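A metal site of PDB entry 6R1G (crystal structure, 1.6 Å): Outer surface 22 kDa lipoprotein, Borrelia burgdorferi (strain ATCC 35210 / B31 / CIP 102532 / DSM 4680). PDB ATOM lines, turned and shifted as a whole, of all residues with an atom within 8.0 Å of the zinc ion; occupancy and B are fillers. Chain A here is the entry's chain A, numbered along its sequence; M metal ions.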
ATOM      1  N   ASP A  26       2.820  14.491   2.063  1.00  0.00           N
ATOM      2  CA  ASP A  26       2.062  15.702   2.450  1.00  0.00           C
ATOM      3  C   ASP A  26       0.629  15.362   2.848  1.00  0.00           C
ATOM      4  O   ASP A  26       0.100  14.264   2.527  1.00  0.00           O
ATOM      5  CB  ASP A  26       2.177  16.788   1.379  1.00  0.00           C
ATOM      6  CG  ASP A  26       1.458  16.526   0.073  1.00  0.00           C
ATOM      7  OD1 ASP A  26       0.674  15.616  -0.018  1.00  0.00           O
ATOM      8  OD2 ASP A  26       1.670  17.329  -0.818  1.00  0.00           O
ATOM      9  N   HIS A  28      -2.164  16.621   1.897  1.00  0.00           N
ATOM     10  CA  HIS A  28      -3.072  16.459   0.739  1.00  0.00           C
ATOM     11  C   HIS A  28      -3.057  14.989   0.257  1.00  0.00           C
ATOM     12  O   HIS A  28      -4.149  14.354   0.021  1.00  0.00           O
ATOM     13  CB  HIS A  28      -2.701  17.437  -0.386  1.00  0.00           C
ATOM     14  CG  HIS A  28      -3.675  17.387  -1.524  1.00  0.00           C
ATOM     15  ND1 HIS A  28      -4.927  17.969  -1.399  1.00  0.00           N
ATOM     16  CD2 HIS A  28      -3.642  16.710  -2.671  1.00  0.00           C
ATOM     17  CE1 HIS A  28      -5.646  17.680  -2.486  1.00  0.00           C
ATOM     18  NE2 HIS A  28      -4.865  16.913  -3.295  1.00  0.00           N
ATOM     19  N   THR A  29      -1.865  14.446   0.068  1.00  0.00           N
ATOM     20  CA  THR A  29      -1.694  13.044  -0.406  1.00  0.00           C
ATOM     21  C   THR A  29      -2.199  12.086   0.643  1.00  0.00           C
ATOM     22  O   THR A  29      -2.927  11.112   0.273  1.00  0.00           O
ATOM     23  CB  THR A  29      -0.245  12.759  -0.785  1.00  0.00           C
ATOM     24  OG1 THR A  29       0.128  13.671  -1.802  1.00  0.00           O
ATOM     25  CG2 THR A  29      -0.064  11.348  -1.300  1.00  0.00           C
ATOM     26  N   GLY A  31      -4.723  12.534   2.471  1.00  0.00           N
ATOM     27  CA  GLY A  31      -6.193  12.501   2.311  1.00  0.00           C
ATOM     28  C   GLY A  31      -6.617  11.581   1.165  1.00  0.00           C
ATOM     29  O   GLY A  31      -7.580  10.821   1.317  1.00  0.00           O
ATOM     30  N   HIS A  32      -5.862  11.602   0.073  1.00  0.00           N
ATOM     31  CA  HIS A  32      -6.103  10.633  -1.032  1.00  0.00           C
ATOM     32  C   HIS A  32      -5.929   9.182  -0.581  1.00  0.00           C
ATOM     33  O   HIS A  32      -6.705   8.285  -0.898  1.00  0.00           O
ATOM     34  CB  HIS A  32      -5.166  10.907  -2.222  1.00  0.00           C
ATOM     35  CG  HIS A  32      -5.536  12.042  -3.096  1.00  0.00           C
ATOM     36  ND1 HIS A  32      -6.487  11.904  -4.050  1.00  0.00           N
ATOM     37  CD2 HIS A  32      -5.084  13.324  -3.156  1.00  0.00           C
ATOM     38  CE1 HIS A  32      -6.645  13.072  -4.640  1.00  0.00           C
ATOM     39  NE2 HIS A  32      -5.759  13.996  -4.114  1.00  0.00           N
ATOM     40  N   PHE A  99      -3.346  11.346 -11.369  1.00  0.00           N
ATOM     41  CA  PHE A  99      -3.018  10.144 -10.586  1.00  0.00           C
ATOM     42  C   PHE A  99      -4.317   9.523 -10.102  1.00  0.00           C
ATOM     43  O   PHE A  99      -5.181  10.219  -9.653  1.00  0.00           O
ATOM     44  CB  PHE A  99      -2.162  10.507  -9.386  1.00  0.00           C
ATOM     45  CG  PHE A  99      -0.764  10.895  -9.746  1.00  0.00           C
ATOM     46  CD1 PHE A  99       0.217   9.919  -9.860  1.00  0.00           C
ATOM     47  CD2 PHE A  99      -0.438  12.220  -9.947  1.00  0.00           C
ATOM     48  CE1 PHE A  99       1.516  10.268 -10.171  1.00  0.00           C
ATOM     49  CE2 PHE A  99       0.870  12.560 -10.299  1.00  0.00           C
ATOM     50  CZ  PHE A  99       1.835  11.585 -10.362  1.00  0.00           C
ATOM     51  N   PHE A 101      -5.712   6.730  -7.205  1.00  0.00           N
ATOM     52  CA  PHE A 101      -5.445   5.984  -5.971  1.00  0.00           C
ATOM     53  C   PHE A 101      -6.542   4.940  -5.837  1.00  0.00           C
ATOM     54  O   PHE A 101      -7.751   5.217  -6.062  1.00  0.00           O
ATOM     55  CB  PHE A 101      -5.534   6.902  -4.754  1.00  0.00           C
ATOM     56  CG  PHE A 101      -4.479   7.960  -4.661  1.00  0.00           C
ATOM     57  CD1 PHE A 101      -4.585   9.104  -5.419  1.00  0.00           C
ATOM     58  CD2 PHE A 101      -3.425   7.837  -3.774  1.00  0.00           C
ATOM     59  CE1 PHE A 101      -3.598  10.082  -5.320  1.00  0.00           C
ATOM     60  CE2 PHE A 101      -2.451   8.810  -3.678  1.00  0.00           C
ATOM     61  CZ  PHE A 101      -2.546   9.933  -4.455  1.00  0.00           C
ATOM     62  N   ASN A 115      -9.982   7.192  -6.057  1.00  0.00           N
ATOM     63  CA  ASN A 115     -10.100   8.644  -6.233  1.00  0.00           C
ATOM     64  C   ASN A 115      -9.022   9.140  -7.190  1.00  0.00           C
ATOM     65  O   ASN A 115      -8.101   8.401  -7.541  1.00  0.00           O
ATOM     66  CB  ASN A 115     -10.085   9.372  -4.886  1.00  0.00           C
ATOM     67  CG  ASN A 115      -8.788   9.196  -4.117  1.00  0.00           C
ATOM     68  OD1 ASN A 115      -7.720   9.592  -4.608  1.00  0.00           O
ATOM     69  ND2 ASN A 115      -8.839   8.523  -2.975  1.00  0.00           N
ATOM     70  N   LEU A 116      -9.181  10.365  -7.684  1.00  0.00           N
ATOM     71  CA  LEU A 116      -8.255  10.999  -8.631  1.00  0.00           C
ATOM     72  C   LEU A 116      -7.649  12.244  -8.006  1.00  0.00           C
ATOM     73  O   LEU A 116      -8.384  13.014  -7.299  1.00  0.00           O
ATOM     74  CB  LEU A 116      -8.951  11.388  -9.930  1.00  0.00           C
ATOM     75  CG  LEU A 116      -9.586  10.257 -10.711  1.00  0.00           C
ATOM     76  CD1 LEU A 116     -10.339  10.852 -11.900  1.00  0.00           C
ATOM     77  CD2 LEU A 116      -8.517   9.305 -11.194  1.00  0.00           C
ATOM     78  N   HIS A 117      -6.398  12.471  -8.333  1.00  0.00           N
ATOM     79  CA  HIS A 117      -5.755  13.780  -8.206  1.00  0.00           C
ATOM     80  C   HIS A 117      -5.456  14.291  -9.609  1.00  0.00           C
ATOM     81  O   HIS A 117      -4.721  13.626 -10.343  1.00  0.00           O
ATOM     82  CB  HIS A 117      -4.483  13.700  -7.343  1.00  0.00           C
ATOM     83  CG  HIS A 117      -3.868  15.042  -7.267  1.00  0.00           C
ATOM     84  ND1 HIS A 117      -4.283  15.978  -6.333  1.00  0.00           N
ATOM     85  CD2 HIS A 117      -2.983  15.657  -8.103  1.00  0.00           C
ATOM     86  CE1 HIS A 117      -3.652  17.120  -6.658  1.00  0.00           C
ATOM     87  NE2 HIS A 117      -2.856  16.950  -7.709  1.00  0.00           N
ATOM     88  N   GLY A 118      -5.963  15.464  -9.964  1.00  0.00           N
ATOM     89  CA  GLY A 118      -5.547  16.118 -11.212  1.00  0.00           C
ATOM     90  C   GLY A 118      -6.586  16.015 -12.282  1.00  0.00           C
ATOM     91  O   GLY A 118      -6.367  16.536 -13.405  1.00  0.00           O
ATOM     92  N   ALA A 119      -7.700  15.405 -11.960  1.00  0.00           N
ATOM     93  CA  ALA A 119      -8.804  15.239 -12.899  1.00  0.00           C
ATOM     94  C   ALA A 119     -10.051  14.944 -12.083  1.00  0.00           C
ATOM     95  O   ALA A 119      -9.969  14.588 -10.906  1.00  0.00           O
ATOM     96  CB  ALA A 119      -8.527  14.146 -13.922  1.00  0.00           C
HETATM   97 ZN    ZN M   1      -5.540  15.841  -4.804  1.00  0.00          ZN
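The zinc ion is bound by a ring nitrogen (NE2) of His 28 (2.0 Å), a ring nitrogen (NE2) of His 32 (2.0 Å) and a ring nitrogen (ND1) of His 117 (2.0 Å).
The zinc ion has three donor atoms within binding distance.
A ring nitrogen (ND1) of His 32 sits at hydrogen-bond distance from the side-chain amide oxygen of Asn 115 (2.7 Å).
N of Phe 99 lies within hydrogen-bond range of O of His 117 (2.9 Å).
Within 4 Å of the zinc ion: His 28, His 32 and His 117.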
